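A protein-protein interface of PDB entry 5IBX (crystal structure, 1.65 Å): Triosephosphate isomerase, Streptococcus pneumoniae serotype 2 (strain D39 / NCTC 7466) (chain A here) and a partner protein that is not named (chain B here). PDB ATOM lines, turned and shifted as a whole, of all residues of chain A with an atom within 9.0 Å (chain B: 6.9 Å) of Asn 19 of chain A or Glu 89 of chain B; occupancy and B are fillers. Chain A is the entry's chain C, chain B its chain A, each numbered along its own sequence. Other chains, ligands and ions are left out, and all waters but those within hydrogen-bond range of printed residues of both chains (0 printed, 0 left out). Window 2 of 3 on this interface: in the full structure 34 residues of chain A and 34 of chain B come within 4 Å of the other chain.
The backbone carbonyl oxygen (O) of Leu 87 of chain B lies within hydrogen-bond range of the side-chain hydroxyl (OG1) of Thr 92 of chain B, 2.8 Å away. The backbone carbonyl oxygen (O) of Lys 18 of chain A sits close to the side-chain carboxylate (OD2) of Asp 50 of chain A (2.6 Å). N of Glu 21 of chain A sits at hydrogen-bond distance from OD1 of Asn 19 of chain A (3.1 Å). The backbone NH (N) of Glu 22 of chain A sits at hydrogen-bond distance from the side-chain amide oxygen (OD1) of Asn 19 of chain A (2.8 Å).
Asn 19 of chain A touches two residues of chain B. Of chain A, only Asn 19 comes within 4 Å of Glu 89 of chain B. Of the printed residues of chain A, Ile 90 of chain B touches Pro 20. Of the printed residues of chain B, Leu 49 of chain A touches Val 86 and Leu 87. Printed residues of chain B within 4 Å of Pro 20 of chain A: Val 86 (3.9 Å) and Ile 90 (3.6 Å). Lys 24 of chain A touches none of the printed residues of chain B. Pro 47 of chain A touches none of the printed residues of chain B. The nearest residue of chain B that does not touch Asn 19 of chain A is Ile 90 of chain B (5.2 Å). The nearest printed residue of chain A that does not touch Ile 90 of chain B is Leu 49 of chain A (4.03 Å).
Of the 11 printed residues of chain B, 4 touch a printed residue of chain A. Hydrophobic or aromatic side chains of chain B within 4 Å of the printed part of chain A: Val 86, Leu 87 and Ile 90. Printed residues of chain A that touch a printed residue of chain B: Lys 18, Asn 19, Pro 20 and Leu 49. Hydrophobic or aromatic side chains of chain A that line the printed part of chain B: Pro 20 and Leu 49. Among the printed residues, no Asp or Glu carboxylate lies within 4 Å of a Lys or Arg side-chain nitrogen of the other chain.
Among the printed residues, pairs that only touch across the chains: Asn 19 of chain A with Glu 89 of chain B, Pro 20 of chain A with Ile 90 of chain B, Leu 49 of chain A with Val 86 of chain B, Asn 19 of chain A with Val 86 of chain B, Leu 49 of chain A with Leu 87 of chain B, Lys 18 of chain A with Val 86 of chain B and Pro 20 of chain A with Val 86 of chain B.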
ATOM      1  N   TRP A  14     -14.801 -13.697  30.562  1.00  0.00           N
ATOM      2  CA  TRP A  14     -14.488 -12.294  30.790  1.00  0.00           C
ATOM      3  C   TRP A  14     -15.688 -11.354  30.777  1.00  0.00           C
ATOM      4  O   TRP A  14     -15.592 -10.231  31.260  1.00  0.00           O
ATOM      5  CB  TRP A  14     -13.474 -11.813  29.778  1.00  0.00           C
ATOM      6  CG  TRP A  14     -12.076 -12.293  29.996  1.00  0.00           C
ATOM      7  CD1 TRP A  14     -11.518 -12.805  31.137  1.00  0.00           C
ATOM      8  CD2 TRP A  14     -11.005 -12.159  29.058  1.00  0.00           C
ATOM      9  NE1 TRP A  14     -10.169 -13.082  30.919  1.00  0.00           N
ATOM     10  CE2 TRP A  14      -9.838 -12.671  29.659  1.00  0.00           C
ATOM     11  CE3 TRP A  14     -10.942 -11.705  27.734  1.00  0.00           C
ATOM     12  CZ2 TRP A  14      -8.590 -12.709  28.986  1.00  0.00           C
ATOM     13  CZ3 TRP A  14      -9.709 -11.754  27.059  1.00  0.00           C
ATOM     14  CH2 TRP A  14      -8.552 -12.266  27.697  1.00  0.00           C
ATOM     15  N   LYS A  15     -16.798 -11.797  30.183  1.00  0.00           N
ATOM     16  CA  LYS A  15     -17.999 -10.987  30.012  1.00  0.00           C
ATOM     17  C   LYS A  15     -17.604  -9.775  29.167  1.00  0.00           C
ATOM     18  O   LYS A  15     -16.748  -9.927  28.309  1.00  0.00           O
ATOM     19  CB  LYS A  15     -18.682 -10.651  31.341  1.00  0.00           C
ATOM     20  CG  LYS A  15     -18.979 -11.922  32.121  1.00  0.00           C
ATOM     21  CD  LYS A  15     -19.878 -11.710  33.334  1.00  0.00           C
ATOM     22  CE  LYS A  15     -20.183 -13.021  34.037  1.00  0.00           C
ATOM     23  NZ  LYS A  15     -21.118 -12.775  35.164  1.00  0.00           N
ATOM     24  N   MET A  16     -18.198  -8.616  29.398  1.00  0.00           N
ATOM     25  CA  MET A  16     -17.918  -7.458  28.549  1.00  0.00           C
ATOM     26  C   MET A  16     -16.786  -6.650  29.180  1.00  0.00           C
ATOM     27  O   MET A  16     -17.007  -5.579  29.731  1.00  0.00           O
ATOM     28  CB  MET A  16     -19.174  -6.623  28.315  1.00  0.00           C
ATOM     29  CG  MET A  16     -18.997  -5.586  27.224  1.00  0.00           C
ATOM     30  SD  MET A  16     -20.405  -4.522  26.915  1.00  0.00           S
ATOM     31  CE  MET A  16     -20.283  -3.475  28.374  1.00  0.00           C
ATOM     32  N   ASN A  17     -15.589  -7.217  29.117  1.00  0.00           N
ATOM     33  CA  ASN A  17     -14.368  -6.615  29.662  1.00  0.00           C
ATOM     34  C   ASN A  17     -13.180  -6.940  28.774  1.00  0.00           C
ATOM     35  O   ASN A  17     -13.107  -8.056  28.191  1.00  0.00           O
ATOM     36  CB  ASN A  17     -14.074  -7.177  31.059  1.00  0.00           C
ATOM     37  CG  ASN A  17     -15.126  -6.781  32.094  1.00  0.00           C
ATOM     38  OD1 ASN A  17     -15.137  -5.649  32.600  1.00  0.00           O
ATOM     39  ND2 ASN A  17     -15.977  -7.742  32.459  1.00  0.00           N
ATOM     40  N   LYS A  18     -12.277  -5.956  28.673  1.00  0.00           N
ATOM     41  CA  LYS A  18     -10.987  -6.023  27.959  1.00  0.00           C
ATOM     42  C   LYS A  18     -11.021  -5.623  26.492  1.00  0.00           C
ATOM     43  O   LYS A  18     -11.921  -6.011  25.751  1.00  0.00           O
ATOM     44  CB  LYS A  18     -10.314  -7.396  28.109  1.00  0.00           C
ATOM     45  CG  LYS A  18     -10.014  -7.755  29.547  1.00  0.00           C
ATOM     46  CD  LYS A  18      -9.155  -8.973  29.650  1.00  0.00           C
ATOM     47  CE  LYS A  18      -9.076  -9.446  31.089  1.00  0.00           C
ATOM     48  NZ  LYS A  18      -8.427  -8.454  31.990  1.00  0.00           N
ATOM     49  N   ASN A  19     -10.047  -4.784  26.119  1.00  0.00           N
ATOM     50  CA  ASN A  19      -9.812  -4.396  24.749  1.00  0.00           C
ATOM     51  C   ASN A  19      -8.761  -5.364  24.201  1.00  0.00           C
ATOM     52  O   ASN A  19      -8.178  -6.167  24.957  1.00  0.00           O
ATOM     53  CB  ASN A  19      -9.365  -2.925  24.610  1.00  0.00           C
ATOM     54  CG  ASN A  19      -8.090  -2.603  25.347  1.00  0.00           C
ATOM     55  OD1 ASN A  19      -7.204  -3.431  25.499  1.00  0.00           O
ATOM     56  ND2 ASN A  19      -8.003  -1.368  25.828  1.00  0.00           N
ATOM     57  N   PRO A  20      -8.502  -5.304  22.907  1.00  0.00           N
ATOM     58  CA  PRO A  20      -7.526  -6.234  22.361  1.00  0.00           C
ATOM     59  C   PRO A  20      -6.135  -6.216  22.997  1.00  0.00           C
ATOM     60  O   PRO A  20      -5.541  -7.285  23.179  1.00  0.00           O
ATOM     61  CB  PRO A  20      -7.491  -5.859  20.883  1.00  0.00           C
ATOM     62  CG  PRO A  20      -8.874  -5.369  20.616  1.00  0.00           C
ATOM     63  CD  PRO A  20      -9.224  -4.579  21.836  1.00  0.00           C
ATOM     64  N   GLU A  21      -5.597  -5.044  23.324  1.00  0.00           N
ATOM     65  CA  GLU A  21      -4.253  -5.011  23.953  1.00  0.00           C
ATOM     66  C   GLU A  21      -4.264  -5.655  25.341  1.00  0.00           C
ATOM     67  O   GLU A  21      -3.296  -6.324  25.716  1.00  0.00           O
ATOM     68  CB  GLU A  21      -3.678  -3.601  23.962  1.00  0.00           C
ATOM     69  CG  GLU A  21      -3.236  -3.119  22.579  1.00  0.00           C
ATOM     70  CD  GLU A  21      -2.167  -4.001  21.931  1.00  0.00           C
ATOM     71  OE1 GLU A  21      -2.240  -4.252  20.707  1.00  0.00           O
ATOM     72  OE2 GLU A  21      -1.232  -4.451  22.631  1.00  0.00           O
ATOM     73  N   GLU A  22      -5.349  -5.446  26.090  1.00  0.00           N
ATOM     74  CA  GLU A  22      -5.514  -6.057  27.412  1.00  0.00           C
ATOM     75  C   GLU A  22      -5.625  -7.560  27.279  1.00  0.00           C
ATOM     76  O   GLU A  22      -4.968  -8.313  28.018  1.00  0.00           O
ATOM     77  CB  GLU A  22      -6.712  -5.466  28.159  1.00  0.00           C
ATOM     78  CG  GLU A  22      -6.477  -4.039  28.655  1.00  0.00           C
ATOM     79  CD  GLU A  22      -7.715  -3.375  29.223  1.00  0.00           C
ATOM     80  OE1 GLU A  22      -8.723  -3.360  28.545  1.00  0.00           O
ATOM     81  OE2 GLU A  22      -7.667  -2.834  30.350  1.00  0.00           O
ATOM     82  N   ALA A  23      -6.402  -7.992  26.287  1.00  0.00           N
ATOM     83  CA  ALA A  23      -6.586  -9.418  26.009  1.00  0.00           C
ATOM     84  C   ALA A  23      -5.253 -10.073  25.600  1.00  0.00           C
ATOM     85  O   ALA A  23      -4.930 -11.171  26.036  1.00  0.00           O
ATOM     86  CB  ALA A  23      -7.605  -9.588  24.905  1.00  0.00           C
ATOM     87  N   LYS A  24      -4.481  -9.383  24.769  1.00  0.00           N
ATOM     88  CA  LYS A  24      -3.152  -9.875  24.352  1.00  0.00           C
ATOM     89  C   LYS A  24      -2.214  -9.997  25.558  1.00  0.00           C
ATOM     90  O   LYS A  24      -1.507 -10.992  25.697  1.00  0.00           O
ATOM     91  CB  LYS A  24      -2.539  -8.936  23.315  1.00  0.00           C
ATOM     92  CG  LYS A  24      -1.088  -9.215  22.938  1.00  0.00           C
ATOM     93  CD  LYS A  24      -0.672  -8.352  21.759  1.00  0.00           C
ATOM     94  CE  LYS A  24       0.736  -8.661  21.272  1.00  0.00           C
ATOM     95  NZ  LYS A  24       1.788  -8.214  22.225  1.00  0.00           N
ATOM     96  N   ALA A  25      -2.201  -8.982  26.418  1.00  0.00           N
ATOM     97  CA  ALA A  25      -1.295  -8.999  27.593  1.00  0.00           C
ATOM     98  C   ALA A  25      -1.635 -10.153  28.535  1.00  0.00           C
ATOM     99  O   ALA A  25      -0.734 -10.815  29.070  1.00  0.00           O
ATOM    100  CB  ALA A  25      -1.332  -7.673  28.331  1.00  0.00           C
ATOM    101  N   PHE A  26      -2.932 -10.415  28.706  1.00  0.00           N
ATOM    102  CA  PHE A  26      -3.386 -11.534  29.555  1.00  0.00           C
ATOM    103  C   PHE A  26      -2.897 -12.878  29.009  1.00  0.00           C
ATOM    104  O   PHE A  26      -2.285 -13.678  29.741  1.00  0.00           O
ATOM    105  CB  PHE A  26      -4.908 -11.531  29.650  1.00  0.00           C
ATOM    106  CG  PHE A  26      -5.501 -12.612  30.532  1.00  0.00           C
ATOM    107  CD1 PHE A  26      -5.624 -13.923  30.083  1.00  0.00           C
ATOM    108  CD2 PHE A  26      -6.044 -12.282  31.764  1.00  0.00           C
ATOM    109  CE1 PHE A  26      -6.211 -14.902  30.877  1.00  0.00           C
ATOM    110  CE2 PHE A  26      -6.658 -13.239  32.546  1.00  0.00           C
ATOM    111  CZ  PHE A  26      -6.741 -14.551  32.110  1.00  0.00           C
ATOM    112  N   VAL A  27      -3.154 -13.116  27.719  1.00  0.00           N
ATOM    113  CA  VAL A  27      -2.767 -14.370  27.072  1.00  0.00           C
ATOM    114  C   VAL A  27      -1.244 -14.534  27.141  1.00  0.00           C
ATOM    115  O   VAL A  27      -0.736 -15.613  27.433  1.00  0.00           O
ATOM    116  CB  VAL A  27      -3.304 -14.447  25.619  1.00  0.00           C
ATOM    117  CG1 VAL A  27      -2.801 -15.693  24.895  1.00  0.00           C
ATOM    118  CG2 VAL A  27      -4.821 -14.433  25.631  1.00  0.00           C
ATOM    119  N   ALA A  46     -13.845 -14.746  25.407  1.00  0.00           N
ATOM    120  CA  ALA A  46     -13.490 -13.327  25.231  1.00  0.00           C
ATOM    121  C   ALA A  46     -14.497 -12.598  24.370  1.00  0.00           C
ATOM    122  O   ALA A  46     -15.196 -13.237  23.567  1.00  0.00           O
ATOM    123  CB  ALA A  46     -12.112 -13.216  24.586  1.00  0.00           C
ATOM    124  N   PRO A  47     -14.566 -11.247  24.515  1.00  0.00           N
ATOM    125  CA  PRO A  47     -15.501 -10.480  23.636  1.00  0.00           C
ATOM    126  C   PRO A  47     -15.207 -10.665  22.139  1.00  0.00           C
ATOM    127  O   PRO A  47     -14.026 -10.895  21.760  1.00  0.00           O
ATOM    128  CB  PRO A  47     -15.225  -9.028  24.032  1.00  0.00           C
ATOM    129  CG  PRO A  47     -14.743  -9.110  25.477  1.00  0.00           C
ATOM    130  CD  PRO A  47     -13.958 -10.396  25.568  1.00  0.00           C
ATOM    131  N   LEU A  49     -14.836  -8.546  19.822  1.00  0.00           N
ATOM    132  CA  LEU A  49     -13.803  -7.576  19.358  1.00  0.00           C
ATOM    133  C   LEU A  49     -12.404  -8.080  19.584  1.00  0.00           C
ATOM    134  O   LEU A  49     -11.487  -7.735  18.832  1.00  0.00           O
ATOM    135  CB  LEU A  49     -13.933  -6.220  20.072  1.00  0.00           C
ATOM    136  CG  LEU A  49     -15.138  -5.385  19.703  1.00  0.00           C
ATOM    137  CD1 LEU A  49     -15.198  -4.152  20.585  1.00  0.00           C
ATOM    138  CD2 LEU A  49     -15.152  -4.979  18.227  1.00  0.00           C
ATOM    139  N   ASP A  50     -12.237  -8.899  20.622  1.00  0.00           N
ATOM    140  CA  ASP A  50     -10.922  -9.402  20.995  1.00  0.00           C
ATOM    141  C   ASP A  50     -10.558 -10.780  20.467  1.00  0.00           C
ATOM    142  O   ASP A  50      -9.428 -11.225  20.660  1.00  0.00           O
ATOM    143  CB  ASP A  50     -10.841  -9.489  22.530  1.00  0.00           C
ATOM    144  CG  ASP A  50     -11.063  -8.166  23.223  1.00  0.00           C
ATOM    145  OD1 ASP A  50     -10.853  -7.079  22.634  1.00  0.00           O
ATOM    146  OD2 ASP A  50     -11.458  -8.231  24.415  1.00  0.00           O
ATOM    147  N   LEU A  51     -11.495 -11.496  19.843  1.00  0.00           N
ATOM    148  CA  LEU A  51     -11.226 -12.911  19.496  1.00  0.00           C
ATOM    149  C   LEU A  51     -10.058 -13.192  18.558  1.00  0.00           C
ATOM    150  O   LEU A  51      -9.274 -14.112  18.832  1.00  0.00           O
ATOM    151  CB  LEU A  51     -12.486 -13.625  19.018  1.00  0.00           C
ATOM    152  CG  LEU A  51     -13.418 -14.155  20.110  1.00  0.00           C
ATOM    153  CD1 LEU A  51     -14.723 -14.697  19.524  1.00  0.00           C
ATOM    154  CD2 LEU A  51     -12.758 -15.245  20.931  1.00  0.00           C
ATOM    155  N   THR A  53      -7.418 -11.446  18.148  1.00  0.00           N
ATOM    156  CA  THR A  53      -6.224 -11.126  18.917  1.00  0.00           C
ATOM    157  C   THR A  53      -5.914 -12.256  19.902  1.00  0.00           C
ATOM    158  O   THR A  53      -4.770 -12.674  19.996  1.00  0.00           O
ATOM    159  CB  THR A  53      -6.324  -9.781  19.690  1.00  0.00           C
ATOM    160  OG1 THR A  53      -6.598  -8.700  18.784  1.00  0.00           O
ATOM    161  CG2 THR A  53      -5.017  -9.486  20.459  1.00  0.00           C
ATOM    162  N   VAL A  54      -6.921 -12.756  20.607  1.00  0.00           N
ATOM    163  CA  VAL A  54      -6.702 -13.848  21.549  1.00  0.00           C
ATOM    164  C   VAL A  54      -6.204 -15.106  20.792  1.00  0.00           C
ATOM    165  O   VAL A  54      -5.287 -15.764  21.227  1.00  0.00           O
ATOM    166  CB  VAL A  54      -7.945 -14.113  22.403  1.00  0.00           C
ATOM    167  CG1 VAL A  54      -7.804 -15.419  23.189  1.00  0.00           C
ATOM    168  CG2 VAL A  54      -8.159 -12.927  23.350  1.00  0.00           C
ATOM    169  N   PRO B  84     -18.874   0.075  23.891  1.00  0.00           N
ATOM    170  CA  PRO B  84     -18.553   1.312  23.140  1.00  0.00           C
ATOM    171  C   PRO B  84     -17.184   1.907  23.558  1.00  0.00           C
ATOM    172  O   PRO B  84     -16.528   2.574  22.761  1.00  0.00           O
ATOM    173  CB  PRO B  84     -19.715   2.265  23.472  1.00  0.00           C
ATOM    174  CG  PRO B  84     -20.291   1.737  24.760  1.00  0.00           C
ATOM    175  CD  PRO B  84     -20.090   0.243  24.711  1.00  0.00           C
ATOM    176  N   GLN B  85     -16.746   1.619  24.775  1.00  0.00           N
ATOM    177  CA  GLN B  85     -15.440   2.064  25.233  1.00  0.00           C
ATOM    178  C   GLN B  85     -14.320   1.387  24.414  1.00  0.00           C
ATOM    179  O   GLN B  85     -13.344   2.050  23.955  1.00  0.00           O
ATOM    180  CB  GLN B  85     -15.270   1.757  26.725  1.00  0.00           C
ATOM    181  CG  GLN B  85     -13.968   2.260  27.294  1.00  0.00           C
ATOM    182  CD  GLN B  85     -13.903   2.176  28.801  1.00  0.00           C
ATOM    183  OE1 GLN B  85     -14.187   1.137  29.391  1.00  0.00           O
ATOM    184  NE2 GLN B  85     -13.495   3.263  29.434  1.00  0.00           N
ATOM    185  N   VAL B  86     -14.419   0.067  24.308  1.00  0.00           N
ATOM    186  CA  VAL B  86     -13.486  -0.710  23.509  1.00  0.00           C
ATOM    187  C   VAL B  86     -13.568  -0.283  22.048  1.00  0.00           C
ATOM    188  O   VAL B  86     -12.512  -0.134  21.410  1.00  0.00           O
ATOM    189  CB  VAL B  86     -13.693  -2.221  23.663  1.00  0.00           C
ATOM    190  CG1 VAL B  86     -12.636  -2.988  22.861  1.00  0.00           C
ATOM    191  CG2 VAL B  86     -13.571  -2.614  25.129  1.00  0.00           C
ATOM    192  N   LEU B  87     -14.787  -0.146  21.505  1.00  0.00           N
ATOM    193  CA  LEU B  87     -14.935   0.335  20.130  1.00  0.00           C
ATOM    194  C   LEU B  87     -14.168   1.619  19.877  1.00  0.00           C
ATOM    195  O   LEU B  87     -13.531   1.757  18.850  1.00  0.00           O
ATOM    196  CB  LEU B  87     -16.373   0.524  19.732  1.00  0.00           C
ATOM    197  CG  LEU B  87     -17.213  -0.724  19.443  1.00  0.00           C
ATOM    198  CD1 LEU B  87     -18.693  -0.364  19.246  1.00  0.00           C
ATOM    199  CD2 LEU B  87     -16.671  -1.467  18.222  1.00  0.00           C
ATOM    200  N   LYS B  88     -14.218   2.553  20.831  1.00  0.00           N
ATOM    201  CA  LYS B  88     -13.540   3.824  20.679  1.00  0.00           C
ATOM    202  C   LYS B  88     -12.009   3.630  20.701  1.00  0.00           C
ATOM    203  O   LYS B  88     -11.293   4.182  19.878  1.00  0.00           O
ATOM    204  CB  LYS B  88     -14.010   4.820  21.741  1.00  0.00           C
ATOM    205  CG  LYS B  88     -13.145   6.090  21.810  1.00  0.00           C
ATOM    206  CD  LYS B  88     -13.197   6.890  20.498  1.00  0.00           C
ATOM    207  CE  LYS B  88     -12.434   8.214  20.601  1.00  0.00           C
ATOM    208  NZ  LYS B  88     -12.636   9.142  19.445  1.00  0.00           N
ATOM    209  N   GLU B  89     -11.531   2.860  21.667  1.00  0.00           N
ATOM    210  CA  GLU B  89     -10.098   2.566  21.839  1.00  0.00           C
ATOM    211  C   GLU B  89      -9.465   1.948  20.585  1.00  0.00           C
ATOM    212  O   GLU B  89      -8.323   2.240  20.284  1.00  0.00           O
ATOM    213  CB  GLU B  89      -9.929   1.581  23.013  1.00  0.00           C
ATOM    214  CG  GLU B  89      -8.506   1.130  23.295  1.00  0.00           C
ATOM    215  CD  GLU B  89      -7.623   2.230  23.832  1.00  0.00           C
ATOM    216  OE1 GLU B  89      -8.134   3.267  24.328  1.00  0.00           O
ATOM    217  OE2 GLU B  89      -6.396   2.038  23.787  1.00  0.00           O
ATOM    218  N   ILE B  90     -10.216   1.107  19.859  1.00  0.00           N
ATOM    219  CA  ILE B  90      -9.674   0.423  18.662  1.00  0.00           C
ATOM    220  C   ILE B  90      -9.721   1.357  17.443  1.00  0.00           C
ATOM    221  O   ILE B  90      -9.076   1.100  16.431  1.00  0.00           O
ATOM    222  CB  ILE B  90     -10.327  -0.973  18.387  1.00  0.00           C
ATOM    223  CG1 ILE B  90     -11.810  -0.863  18.052  1.00  0.00           C
ATOM    224  CG2 ILE B  90     -10.123  -1.929  19.578  1.00  0.00           C
ATOM    225  CD1 ILE B  90     -12.386  -2.140  17.505  1.00  0.00           C
ATOM    226  N   GLY B  91     -10.451   2.460  17.558  1.00  0.00           N
ATOM    227  CA  GLY B  91     -10.493   3.478  16.497  1.00  0.00           C
ATOM    228  C   GLY B  91     -11.755   3.605  15.685  1.00  0.00           C
ATOM    229  O   GLY B  91     -11.730   4.253  14.631  1.00  0.00           O
ATOM    230  N   THR B  92     -12.862   3.027  16.166  1.00  0.00           N
ATOM    231  CA  THR B  92     -14.155   3.028  15.453  1.00  0.00           C
ATOM    232  C   THR B  92     -14.690   4.432  15.359  1.00  0.00           C
ATOM    233  O   THR B  92     -14.525   5.200  16.301  1.00  0.00           O
ATOM    234  CB  THR B  92     -15.200   2.173  16.215  1.00  0.00           C
ATOM    235  OG1 THR B  92     -14.670   0.864  16.456  1.00  0.00           O
ATOM    236  CG2 THR B  92     -16.468   2.033  15.418  1.00  0.00           C
ATOM    237  N   ASN B 123     -18.344   8.082  24.718  1.00  0.00           N
ATOM    238  CA  ASN B 123     -17.122   7.407  24.251  1.00  0.00           C
ATOM    239  C   ASN B 123     -16.541   8.021  22.977  1.00  0.00           C
ATOM    240  O   ASN B 123     -15.776   7.379  22.279  1.00  0.00           O
ATOM    241  CB  ASN B 123     -17.357   5.903  24.145  1.00  0.00           C
ATOM    242  CG  ASN B 123     -17.373   5.236  25.495  1.00  0.00           C
ATOM    243  OD1 ASN B 123     -16.335   5.126  26.146  1.00  0.00           O
ATOM    244  ND2 ASN B 123     -18.558   4.847  25.961  1.00  0.00           N
ATOM    245  N   MET B 125     -17.611   8.823  19.945  1.00  0.00           N
ATOM    246  CA  MET B 125     -17.914   8.325  18.617  1.00  0.00           C
ATOM    247  C   MET B 125     -19.222   8.947  18.196  1.00  0.00           C
ATOM    248  O   MET B 125     -19.751   9.789  18.900  1.00  0.00           O
ATOM    249  CB  MET B 125     -17.978   6.806  18.587  1.00  0.00           C
ATOM    250  CG  MET B 125     -16.684   6.068  18.856  1.00  0.00           C
ATOM    251  SD  MET B 125     -16.935   4.277  18.950  1.00  0.00           S
ATOM    252  CE  MET B 125     -18.190   4.090  20.217  1.00  0.00           C
